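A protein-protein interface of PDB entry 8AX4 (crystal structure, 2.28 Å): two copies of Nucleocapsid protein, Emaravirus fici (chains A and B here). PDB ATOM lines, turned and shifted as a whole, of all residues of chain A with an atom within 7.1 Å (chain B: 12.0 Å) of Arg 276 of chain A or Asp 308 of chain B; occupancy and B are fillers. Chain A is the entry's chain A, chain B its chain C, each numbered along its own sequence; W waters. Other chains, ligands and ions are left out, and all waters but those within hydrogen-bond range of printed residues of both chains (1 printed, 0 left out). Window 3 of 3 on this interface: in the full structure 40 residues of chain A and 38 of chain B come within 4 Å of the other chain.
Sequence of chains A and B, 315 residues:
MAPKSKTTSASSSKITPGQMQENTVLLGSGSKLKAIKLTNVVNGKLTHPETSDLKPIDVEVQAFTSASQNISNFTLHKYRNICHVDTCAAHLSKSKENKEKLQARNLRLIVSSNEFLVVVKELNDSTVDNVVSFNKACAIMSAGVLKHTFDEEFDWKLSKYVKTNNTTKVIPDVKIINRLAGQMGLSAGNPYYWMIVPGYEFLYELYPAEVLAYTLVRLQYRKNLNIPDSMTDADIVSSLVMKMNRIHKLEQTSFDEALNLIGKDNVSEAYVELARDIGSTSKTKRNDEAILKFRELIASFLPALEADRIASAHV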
ATOM      1  N   MET A 184     -19.435 -29.010  26.891  1.00  0.00           N
ATOM      2  CA  MET A 184     -18.953 -29.370  25.564  1.00  0.00           C
ATOM      3  C   MET A 184     -19.044 -28.221  24.568  1.00  0.00           C
ATOM      4  O   MET A 184     -18.483 -28.325  23.472  1.00  0.00           O
ATOM      5  CB  MET A 184     -19.741 -30.575  25.027  1.00  0.00           C
ATOM      6  CG  MET A 184     -18.956 -31.462  24.088  1.00  0.00           C
ATOM      7  SD  MET A 184     -19.961 -32.814  23.432  1.00  0.00           S
ATOM      8  CE  MET A 184     -19.489 -32.822  21.702  1.00  0.00           C
ATOM      9  N   GLY A 185     -19.730 -27.137  24.912  1.00  0.00           N
ATOM     10  CA  GLY A 185     -19.888 -26.029  23.996  1.00  0.00           C
ATOM     11  C   GLY A 185     -21.156 -26.053  23.179  1.00  0.00           C
ATOM     12  O   GLY A 185     -21.297 -25.236  22.263  1.00  0.00           O
ATOM     13  N   VAL A 217     -14.638 -37.353  19.640  1.00  0.00           N
ATOM     14  CA  VAL A 217     -14.400 -36.079  20.306  1.00  0.00           C
ATOM     15  C   VAL A 217     -14.011 -36.303  21.761  1.00  0.00           C
ATOM     16  O   VAL A 217     -13.181 -35.573  22.317  1.00  0.00           O
ATOM     17  CB  VAL A 217     -15.638 -35.176  20.178  1.00  0.00           C
ATOM     18  CG1 VAL A 217     -15.328 -33.833  20.714  1.00  0.00           C
ATOM     19  CG2 VAL A 217     -16.046 -35.038  18.730  1.00  0.00           C
ATOM     20  N   TYR A 221     -10.396 -34.639  22.811  1.00  0.00           N
ATOM     21  CA  TYR A 221     -10.539 -33.477  23.688  1.00  0.00           C
ATOM     22  C   TYR A 221     -10.951 -33.872  25.100  1.00  0.00           C
ATOM     23  O   TYR A 221     -11.762 -33.189  25.730  1.00  0.00           O
ATOM     24  CB  TYR A 221     -11.538 -32.490  23.092  1.00  0.00           C
ATOM     25  CG  TYR A 221     -11.237 -32.106  21.661  1.00  0.00           C
ATOM     26  CD1 TYR A 221     -10.321 -31.103  21.369  1.00  0.00           C
ATOM     27  CD2 TYR A 221     -11.862 -32.750  20.602  1.00  0.00           C
ATOM     28  CE1 TYR A 221     -10.041 -30.750  20.061  1.00  0.00           C
ATOM     29  CE2 TYR A 221     -11.589 -32.404  19.292  1.00  0.00           C
ATOM     30  CZ  TYR A 221     -10.677 -31.403  19.027  1.00  0.00           C
ATOM     31  OH  TYR A 221     -10.402 -31.057  17.724  1.00  0.00           O
ATOM     32  N   GLU A 269     -18.656 -35.387   8.986  1.00  0.00           N
ATOM     33  CA  GLU A 269     -19.630 -34.315   9.152  1.00  0.00           C
ATOM     34  C   GLU A 269     -19.965 -34.105  10.622  1.00  0.00           C
ATOM     35  O   GLU A 269     -19.828 -32.999  11.158  1.00  0.00           O
ATOM     36  CB  GLU A 269     -20.895 -34.642   8.352  1.00  0.00           C
ATOM     37  CG  GLU A 269     -21.526 -33.451   7.661  1.00  0.00           C
ATOM     38  CD  GLU A 269     -22.676 -33.846   6.754  1.00  0.00           C
ATOM     39  OE1 GLU A 269     -22.492 -34.764   5.927  1.00  0.00           O
ATOM     40  OE2 GLU A 269     -23.762 -33.235   6.862  1.00  0.00           O
ATOM     41  N   ALA A 270     -20.401 -35.173  11.290  1.00  0.00           N
ATOM     42  CA  ALA A 270     -20.714 -35.074  12.710  1.00  0.00           C
ATOM     43  C   ALA A 270     -19.480 -34.699  13.520  1.00  0.00           C
ATOM     44  O   ALA A 270     -19.572 -33.916  14.473  1.00  0.00           O
ATOM     45  CB  ALA A 270     -21.307 -36.391  13.207  1.00  0.00           C
ATOM     46  N   TYR A 271     -18.313 -35.234  13.147  1.00  0.00           N
ATOM     47  CA  TYR A 271     -17.099 -34.931  13.900  1.00  0.00           C
ATOM     48  C   TYR A 271     -16.777 -33.442  13.861  1.00  0.00           C
ATOM     49  O   TYR A 271     -16.420 -32.853  14.887  1.00  0.00           O
ATOM     50  CB  TYR A 271     -15.913 -35.744  13.375  1.00  0.00           C
ATOM     51  CG  TYR A 271     -14.607 -35.294  13.987  1.00  0.00           C
ATOM     52  CD1 TYR A 271     -14.220 -35.738  15.241  1.00  0.00           C
ATOM     53  CD2 TYR A 271     -13.772 -34.407  13.326  1.00  0.00           C
ATOM     54  CE1 TYR A 271     -13.042 -35.315  15.812  1.00  0.00           C
ATOM     55  CE2 TYR A 271     -12.586 -33.979  13.893  1.00  0.00           C
ATOM     56  CZ  TYR A 271     -12.225 -34.433  15.134  1.00  0.00           C
ATOM     57  OH  TYR A 271     -11.040 -34.000  15.688  1.00  0.00           O
ATOM     58  N   VAL A 272     -16.893 -32.812  12.688  1.00  0.00           N
ATOM     59  CA  VAL A 272     -16.551 -31.395  12.570  1.00  0.00           C
ATOM     60  C   VAL A 272     -17.514 -30.544  13.383  1.00  0.00           C
ATOM     61  O   VAL A 272     -17.108 -29.594  14.062  1.00  0.00           O
ATOM     62  CB  VAL A 272     -16.542 -30.947  11.099  1.00  0.00           C
ATOM     63  CG1 VAL A 272     -16.057 -29.506  11.002  1.00  0.00           C
ATOM     64  CG2 VAL A 272     -15.698 -31.876  10.243  1.00  0.00           C
ATOM     65  N   GLU A 273     -18.808 -30.855  13.294  1.00  0.00           N
ATOM     66  CA  GLU A 273     -19.809 -30.149  14.084  1.00  0.00           C
ATOM     67  C   GLU A 273     -19.450 -30.173  15.563  1.00  0.00           C
ATOM     68  O   GLU A 273     -19.322 -29.125  16.207  1.00  0.00           O
ATOM     69  CB  GLU A 273     -21.189 -30.774  13.856  1.00  0.00           C
ATOM     70  CG  GLU A 273     -22.349 -29.805  14.032  1.00  0.00           C
ATOM     71  CD  GLU A 273     -23.527 -30.133  13.137  1.00  0.00           C
ATOM     72  OE1 GLU A 273     -24.648 -29.663  13.432  1.00  0.00           O
ATOM     73  OE2 GLU A 273     -23.336 -30.868  12.145  1.00  0.00           O
ATOM     74  N   LEU A 274     -19.257 -31.373  16.112  1.00  0.00           N
ATOM     75  CA  LEU A 274     -18.976 -31.496  17.538  1.00  0.00           C
ATOM     76  C   LEU A 274     -17.608 -30.923  17.894  1.00  0.00           C
ATOM     77  O   LEU A 274     -17.442 -30.328  18.965  1.00  0.00           O
ATOM     78  CB  LEU A 274     -19.083 -32.959  17.956  1.00  0.00           C
ATOM     79  CG  LEU A 274     -20.456 -33.558  17.650  1.00  0.00           C
ATOM     80  CD1 LEU A 274     -20.450 -35.073  17.773  1.00  0.00           C
ATOM     81  CD2 LEU A 274     -21.511 -32.943  18.556  1.00  0.00           C
ATOM     82  N   ALA A 275     -16.619 -31.078  17.007  1.00  0.00           N
ATOM     83  CA  ALA A 275     -15.262 -30.650  17.343  1.00  0.00           C
ATOM     84  C   ALA A 275     -15.107 -29.135  17.296  1.00  0.00           C
ATOM     85  O   ALA A 275     -14.301 -28.578  18.054  1.00  0.00           O
ATOM     86  CB  ALA A 275     -14.247 -31.315  16.415  1.00  0.00           C
ATOM     87  N   ARG A 276     -15.858 -28.456  16.420  1.00  0.00           N
ATOM     88  CA  ARG A 276     -15.714 -27.006  16.310  1.00  0.00           C
ATOM     89  C   ARG A 276     -16.249 -26.304  17.552  1.00  0.00           C
ATOM     90  O   ARG A 276     -15.642 -25.350  18.042  1.00  0.00           O
ATOM     91  CB  ARG A 276     -16.400 -26.482  15.042  1.00  0.00           C
ATOM     92  CG  ARG A 276     -17.921 -26.540  14.982  1.00  0.00           C
ATOM     93  CD  ARG A 276     -18.423 -25.556  13.919  1.00  0.00           C
ATOM     94  NE  ARG A 276     -19.846 -25.708  13.663  1.00  0.00           N
ATOM     95  CZ  ARG A 276     -20.341 -26.408  12.649  1.00  0.00           C
ATOM     96  NH1 ARG A 276     -19.524 -26.997  11.788  1.00  0.00           N
ATOM     97  NH2 ARG A 276     -21.655 -26.500  12.490  1.00  0.00           N
ATOM     98  N   ASP A 277     -17.364 -26.782  18.099  1.00  0.00           N
ATOM     99  CA  ASP A 277     -17.933 -26.158  19.292  1.00  0.00           C
ATOM    100  C   ASP A 277     -17.016 -26.305  20.495  1.00  0.00           C
ATOM    101  O   ASP A 277     -17.035 -25.459  21.395  1.00  0.00           O
ATOM    102  CB  ASP A 277     -19.316 -26.749  19.606  1.00  0.00           C
ATOM    103  CG  ASP A 277     -20.312 -26.538  18.479  1.00  0.00           C
ATOM    104  OD1 ASP A 277     -20.412 -25.391  17.984  1.00  0.00           O
ATOM    105  OD2 ASP A 277     -21.019 -27.496  18.119  1.00  0.00           O
ATOM    106  N   ILE A 278     -16.210 -27.368  20.532  1.00  0.00           N
ATOM    107  CA  ILE A 278     -15.233 -27.509  21.605  1.00  0.00           C
ATOM    108  C   ILE A 278     -14.098 -26.510  21.426  1.00  0.00           C
ATOM    109  O   ILE A 278     -13.701 -25.821  22.374  1.00  0.00           O
ATOM    110  CB  ILE A 278     -14.695 -28.946  21.671  1.00  0.00           C
ATOM    111  CG1 ILE A 278     -15.855 -29.923  21.766  1.00  0.00           C
ATOM    112  CG2 ILE A 278     -13.727 -29.093  22.845  1.00  0.00           C
ATOM    113  CD1 ILE A 278     -15.496 -31.183  22.420  1.00  0.00           C
ATOM    114  N   GLY A 279     -13.550 -26.430  20.210  1.00  0.00           N
ATOM    115  CA  GLY A 279     -12.438 -25.524  19.963  1.00  0.00           C
ATOM    116  C   GLY A 279     -12.732 -24.099  20.376  1.00  0.00           C
ATOM    117  O   GLY A 279     -11.977 -23.492  21.139  1.00  0.00           O
ATOM    118  N   SER A 280     -13.858 -23.556  19.906  1.00  0.00           N
ATOM    119  CA  SER A 280     -14.240 -22.189  20.246  1.00  0.00           C
ATOM    120  C   SER A 280     -14.564 -22.035  21.729  1.00  0.00           C
ATOM    121  O   SER A 280     -14.542 -20.914  22.247  1.00  0.00           O
ATOM    122  CB  SER A 280     -15.434 -21.730  19.407  1.00  0.00           C
ATOM    123  OG  SER A 280     -16.343 -22.797  19.170  1.00  0.00           O
ATOM    124  N   THR A 281     -14.863 -23.134  22.423  1.00  0.00           N
ATOM    125  CA  THR A 281     -15.227 -23.103  23.836  1.00  0.00           C
ATOM    126  C   THR A 281     -14.016 -23.152  24.764  1.00  0.00           C
ATOM    127  O   THR A 281     -14.104 -22.681  25.904  1.00  0.00           O
ATOM    128  CB  THR A 281     -16.185 -24.273  24.140  1.00  0.00           C
ATOM    129  OG1 THR A 281     -17.445 -24.034  23.495  1.00  0.00           O
ATOM    130  CG2 THR A 281     -16.428 -24.453  25.629  1.00  0.00           C
ATOM    131  N   SER A 282     -12.878 -23.660  24.288  1.00  0.00           N
ATOM    132  CA  SER A 282     -11.737 -23.942  25.155  1.00  0.00           C
ATOM    133  C   SER A 282     -11.195 -22.669  25.802  1.00  0.00           C
ATOM    134  O   SER A 282     -10.785 -21.731  25.110  1.00  0.00           O
ATOM    135  CB  SER A 282     -10.638 -24.641  24.359  1.00  0.00           C
ATOM    136  OG  SER A 282      -9.581 -25.061  25.204  1.00  0.00           O
ATOM    137  N   LYS A 285      -7.352 -22.588  25.200  1.00  0.00           N
ATOM    138  CA  LYS A 285      -6.980 -22.161  23.855  1.00  0.00           C
ATOM    139  C   LYS A 285      -7.054 -20.645  23.718  1.00  0.00           C
ATOM    140  O   LYS A 285      -6.144 -20.015  23.165  1.00  0.00           O
ATOM    141  CB  LYS A 285      -7.891 -22.845  22.840  1.00  0.00           C
ATOM    142  CG  LYS A 285      -7.514 -22.655  21.389  1.00  0.00           C
ATOM    143  CD  LYS A 285      -8.366 -23.564  20.524  1.00  0.00           C
ATOM    144  CE  LYS A 285      -8.199 -23.249  19.053  1.00  0.00           C
ATOM    145  NZ  LYS A 285      -9.267 -23.870  18.224  1.00  0.00           N
ATOM    146  N   ILE B 298      -9.479 -39.411  12.976  1.00  0.00           N
ATOM    147  CA  ILE B 298      -9.319 -38.024  13.412  1.00  0.00           C
ATOM    148  C   ILE B 298      -8.337 -37.293  12.508  1.00  0.00           C
ATOM    149  O   ILE B 298      -8.540 -36.121  12.162  1.00  0.00           O
ATOM    150  CB  ILE B 298      -8.879 -37.979  14.888  1.00  0.00           C
ATOM    151  CG1 ILE B 298      -9.975 -38.557  15.784  1.00  0.00           C
ATOM    152  CG2 ILE B 298      -8.543 -36.556  15.307  1.00  0.00           C
ATOM    153  CD1 ILE B 298      -9.511 -38.872  17.186  1.00  0.00           C
ATOM    154  N   SER B 300      -7.744 -38.111   9.307  1.00  0.00           N
ATOM    155  CA  SER B 300      -8.477 -37.945   8.053  1.00  0.00           C
ATOM    156  C   SER B 300      -9.266 -36.644   8.036  1.00  0.00           C
ATOM    157  O   SER B 300      -9.332 -35.956   7.009  1.00  0.00           O
ATOM    158  CB  SER B 300      -9.435 -39.120   7.848  1.00  0.00           C
ATOM    159  OG  SER B 300      -8.761 -40.320   7.523  1.00  0.00           O
ATOM    160  N   PHE B 301      -9.843 -36.277   9.180  1.00  0.00           N
ATOM    161  CA  PHE B 301     -10.835 -35.217   9.253  1.00  0.00           C
ATOM    162  C   PHE B 301     -10.226 -33.833   9.432  1.00  0.00           C
ATOM    163  O   PHE B 301     -10.967 -32.844   9.412  1.00  0.00           O
ATOM    164  CB  PHE B 301     -11.811 -35.503  10.397  1.00  0.00           C
ATOM    165  CG  PHE B 301     -12.548 -36.810  10.257  1.00  0.00           C
ATOM    166  CD1 PHE B 301     -12.675 -37.424   9.022  1.00  0.00           C
ATOM    167  CD2 PHE B 301     -13.105 -37.431  11.365  1.00  0.00           C
ATOM    168  CE1 PHE B 301     -13.345 -38.625   8.892  1.00  0.00           C
ATOM    169  CE2 PHE B 301     -13.777 -38.632  11.240  1.00  0.00           C
ATOM    170  CZ  PHE B 301     -13.898 -39.230  10.003  1.00  0.00           C
ATOM    171  N   LEU B 302      -8.906 -33.736   9.600  1.00  0.00           N
ATOM    172  CA  LEU B 302      -8.283 -32.427   9.783  1.00  0.00           C
ATOM    173  C   LEU B 302      -8.475 -31.500   8.587  1.00  0.00           C
ATOM    174  O   LEU B 302      -8.676 -30.293   8.811  1.00  0.00           O
ATOM    175  CB  LEU B 302      -6.795 -32.597  10.114  1.00  0.00           C
ATOM    176  CG  LEU B 302      -6.063 -31.295  10.441  1.00  0.00           C
ATOM    177  CD1 LEU B 302      -6.669 -30.657  11.677  1.00  0.00           C
ATOM    178  CD2 LEU B 302      -4.577 -31.540  10.639  1.00  0.00           C
ATOM    179  N   PRO B 303      -8.412 -31.960   7.328  1.00  0.00           N
ATOM    180  CA  PRO B 303      -8.833 -31.079   6.224  1.00  0.00           C
ATOM    181  C   PRO B 303     -10.216 -30.484   6.434  1.00  0.00           C
ATOM    182  O   PRO B 303     -10.380 -29.259   6.361  1.00  0.00           O
ATOM    183  CB  PRO B 303      -8.786 -32.012   5.009  1.00  0.00           C
ATOM    184  CG  PRO B 303      -7.722 -32.988   5.332  1.00  0.00           C
ATOM    185  CD  PRO B 303      -7.746 -33.179   6.828  1.00  0.00           C
ATOM    186  N   ALA B 304     -11.214 -31.325   6.721  1.00  0.00           N
ATOM    187  CA  ALA B 304     -12.582 -30.840   6.868  1.00  0.00           C
ATOM    188  C   ALA B 304     -12.723 -29.884   8.044  1.00  0.00           C
ATOM    189  O   ALA B 304     -13.538 -28.956   7.989  1.00  0.00           O
ATOM    190  CB  ALA B 304     -13.545 -32.016   7.023  1.00  0.00           C
ATOM    191  N   LEU B 305     -11.944 -30.081   9.111  1.00  0.00           N
ATOM    192  CA  LEU B 305     -12.069 -29.173  10.245  1.00  0.00           C
ATOM    193  C   LEU B 305     -11.428 -27.825   9.937  1.00  0.00           C
ATOM    194  O   LEU B 305     -11.998 -26.782  10.272  1.00  0.00           O
ATOM    195  CB  LEU B 305     -11.468 -29.798  11.506  1.00  0.00           C
ATOM    196  CG  LEU B 305     -11.224 -28.980  12.777  1.00  0.00           C
ATOM    197  CD1 LEU B 305     -12.499 -28.755  13.566  1.00  0.00           C
ATOM    198  CD2 LEU B 305     -10.214 -29.732  13.623  1.00  0.00           C
ATOM    199  N   GLU B 306     -10.261 -27.820   9.274  1.00  0.00           N
ATOM    200  CA  GLU B 306      -9.644 -26.553   8.882  1.00  0.00           C
ATOM    201  C   GLU B 306     -10.505 -25.810   7.872  1.00  0.00           C
ATOM    202  O   GLU B 306     -10.678 -24.591   7.976  1.00  0.00           O
ATOM    203  CB  GLU B 306      -8.241 -26.768   8.306  1.00  0.00           C
ATOM    204  CG  GLU B 306      -7.263 -27.506   9.207  1.00  0.00           C
ATOM    205  CD  GLU B 306      -6.589 -26.603  10.233  1.00  0.00           C
ATOM    206  OE1 GLU B 306      -7.278 -25.738  10.816  1.00  0.00           O
ATOM    207  OE2 GLU B 306      -5.380 -26.786  10.492  1.00  0.00           O
ATOM    208  N   ALA B 307     -11.036 -26.524   6.877  1.00  0.00           N
ATOM    209  CA  ALA B 307     -11.971 -25.908   5.945  1.00  0.00           C
ATOM    210  C   ALA B 307     -13.131 -25.256   6.686  1.00  0.00           C
ATOM    211  O   ALA B 307     -13.563 -24.151   6.337  1.00  0.00           O
ATOM    212  CB  ALA B 307     -12.485 -26.952   4.953  1.00  0.00           C
ATOM    213  N   ASP B 308     -13.627 -25.916   7.734  1.00  0.00           N
ATOM    214  CA  ASP B 308     -14.780 -25.399   8.461  1.00  0.00           C
ATOM    215  C   ASP B 308     -14.429 -24.181   9.305  1.00  0.00           C
ATOM    216  O   ASP B 308     -15.292 -23.329   9.541  1.00  0.00           O
ATOM    217  CB  ASP B 308     -15.373 -26.492   9.346  1.00  0.00           C
ATOM    218  CG  ASP B 308     -16.736 -26.126   9.896  1.00  0.00           C
ATOM    219  OD1 ASP B 308     -16.793 -25.434  10.936  1.00  0.00           O
ATOM    220  OD2 ASP B 308     -17.749 -26.532   9.288  1.00  0.00           O
ATOM    221  N   ARG B 309     -13.181 -24.069   9.767  1.00  0.00           N
ATOM    222  CA  ARG B 309     -12.857 -22.988  10.693  1.00  0.00           C
ATOM    223  C   ARG B 309     -12.717 -21.642   9.997  1.00  0.00           C
ATOM    224  O   ARG B 309     -13.184 -20.629  10.527  1.00  0.00           O
ATOM    225  CB  ARG B 309     -11.579 -23.293  11.467  1.00  0.00           C
ATOM    226  CG  ARG B 309     -11.711 -24.425  12.441  1.00  0.00           C
ATOM    227  CD  ARG B 309     -10.440 -25.244  12.428  1.00  0.00           C
ATOM    228  NE  ARG B 309      -9.586 -24.917  13.564  1.00  0.00           N
ATOM    229  CZ  ARG B 309      -8.612 -25.704  14.003  1.00  0.00           C
ATOM    230  NH1 ARG B 309      -8.358 -26.858  13.405  1.00  0.00           N
ATOM    231  NH2 ARG B 309      -7.887 -25.333  15.034  1.00  0.00           N
ATOM    232  N   ILE B 310     -12.070 -21.588   8.833  1.00  0.00           N
ATOM    233  CA  ILE B 310     -11.924 -20.291   8.182  1.00  0.00           C
ATOM    234  C   ILE B 310     -13.244 -19.852   7.556  1.00  0.00           C
ATOM    235  O   ILE B 310     -13.560 -18.657   7.540  1.00  0.00           O
ATOM    236  CB  ILE B 310     -10.779 -20.312   7.155  1.00  0.00           C
ATOM    237  CG1 ILE B 310     -10.995 -21.426   6.131  1.00  0.00           C
ATOM    238  CG2 ILE B 310      -9.446 -20.484   7.861  1.00  0.00           C
ATOM    239  CD1 ILE B 310      -9.886 -21.546   5.120  1.00  0.00           C
ATOM    240  N   ALA B 311     -14.034 -20.801   7.040  1.00  0.00           N
ATOM    241  CA  ALA B 311     -15.415 -20.499   6.671  1.00  0.00           C
ATOM    242  C   ALA B 311     -16.114 -19.746   7.796  1.00  0.00           C
ATOM    243  O   ALA B 311     -16.780 -18.731   7.566  1.00  0.00           O
ATOM    244  CB  ALA B 311     -16.165 -21.791   6.339  1.00  0.00           C
ATOM    245  N   SER B 312     -15.959 -20.228   9.025  1.00  0.00           N
ATOM    246  CA  SER B 312     -16.332 -19.478  10.214  1.00  0.00           C
ATOM    247  C   SER B 312     -15.288 -18.409  10.517  1.00  0.00           C
ATOM    248  O   SER B 312     -15.402 -17.270  10.067  1.00  0.00           O
ATOM    249  CB  SER B 312     -16.488 -20.414  11.415  1.00  0.00           C
ATOM    250  OG  SER B 312     -16.138 -19.758  12.621  1.00  0.00           O
HETATM  251  O   HOH W   1      -8.800 -33.662  13.057  1.00  0.00           O
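Arg 276 of chain A touches just one residue of chain B: Asp 308.
Asp 308 of chain B touches just these residues of chain A: Val 272 (3.5 Å) and Arg 276 (3.1 Å).
Of chain B, only Ile 298 and Phe 301 come within 4 Å of Tyr 271 of chain A.
Val 272 of chain A touches just these residues of chain B: Ala 304 (3.9 Å) and Asp 308 (3.5 Å).
Asp 277 of chain A touches none of the printed residues of chain B.
No residue of chain B comes within 4 Å of Gly 279 of chain A.
No residue of chain B comes within 4 Å of Ser 280 of chain A.
Of the printed residues of chain A, Ile 298 of chain B touches Tyr 271 (3.6 Å).
Of the printed residues of chain A, Phe 301 of chain B touches Tyr 271.
Tyr 221 of chain A touches none of the printed residues of chain B.
The nearest residue of chain A that does not touch Asp 308 of chain B is Glu 273 of chain A (6.0 Å).
The nearest printed residue of chain A that does not touch Arg 309 of chain B is Arg 276 of chain A (5.7 Å).
The side-chain carboxylate (OE1) of Glu 306 of chain B is in salt-bridge range of the guanidinium group (NH1) of Arg 309 of chain B, 3.0 Å away.
N of Lys 285 of chain A lies within hydrogen-bond range of OG of Ser 282 of chain A, 3.3 Å away.
The backbone carbonyl oxygen (O) of Arg 276 of chain A lies within hydrogen-bond range of the side-chain hydroxyl (OG) of Ser 280 of chain A, 2.9 Å away.
Of the 14 printed residues of chain B, 5 touch a printed residue of chain A.
Hydrophobic or aromatic side chains of chain B that line the printed part of chain A: Ile 298, Phe 301 and Ala 304.
Along chain A the printed residues that touch a printed residue of chain B span positions 271 to 285.
Among the printed residues, 6 pairs touch across the chains.
Water W1 lies within hydrogen-bond range of the backbone carbonyl oxygen of Ile 298 of chain B (2.6 Å), the backbone NH of Leu 302 of chain B (3.5 Å) and the side-chain hydroxyl of Tyr 271 of chain A (3.5 Å).
The guanidinium group (NH1) of Arg 276 of chain A lies within salt-bridge range of the side-chain carboxylate (OD2) of Asp 308 of chain B (3.1 Å).
CG2 of Ile 298 of chain B touches OH of Tyr 271 of chain A (3.6 Å).
Tyr 271 of chain A touches Phe 301 of chain B (CD2 to CD2, 3.7 Å).
Val 272 of chain A touches Ala 304 of chain B.
Val 272 of chain A touches Asp 308 of chain B (CG1 to CB, 3.5 Å).
Lys 285 of chain A touches Arg 309 of chain B.
No position is printed for both chains.
Of the 6 pairs that touch across the chains among the printed residues, none has its exchanged pair printed and touching as well.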
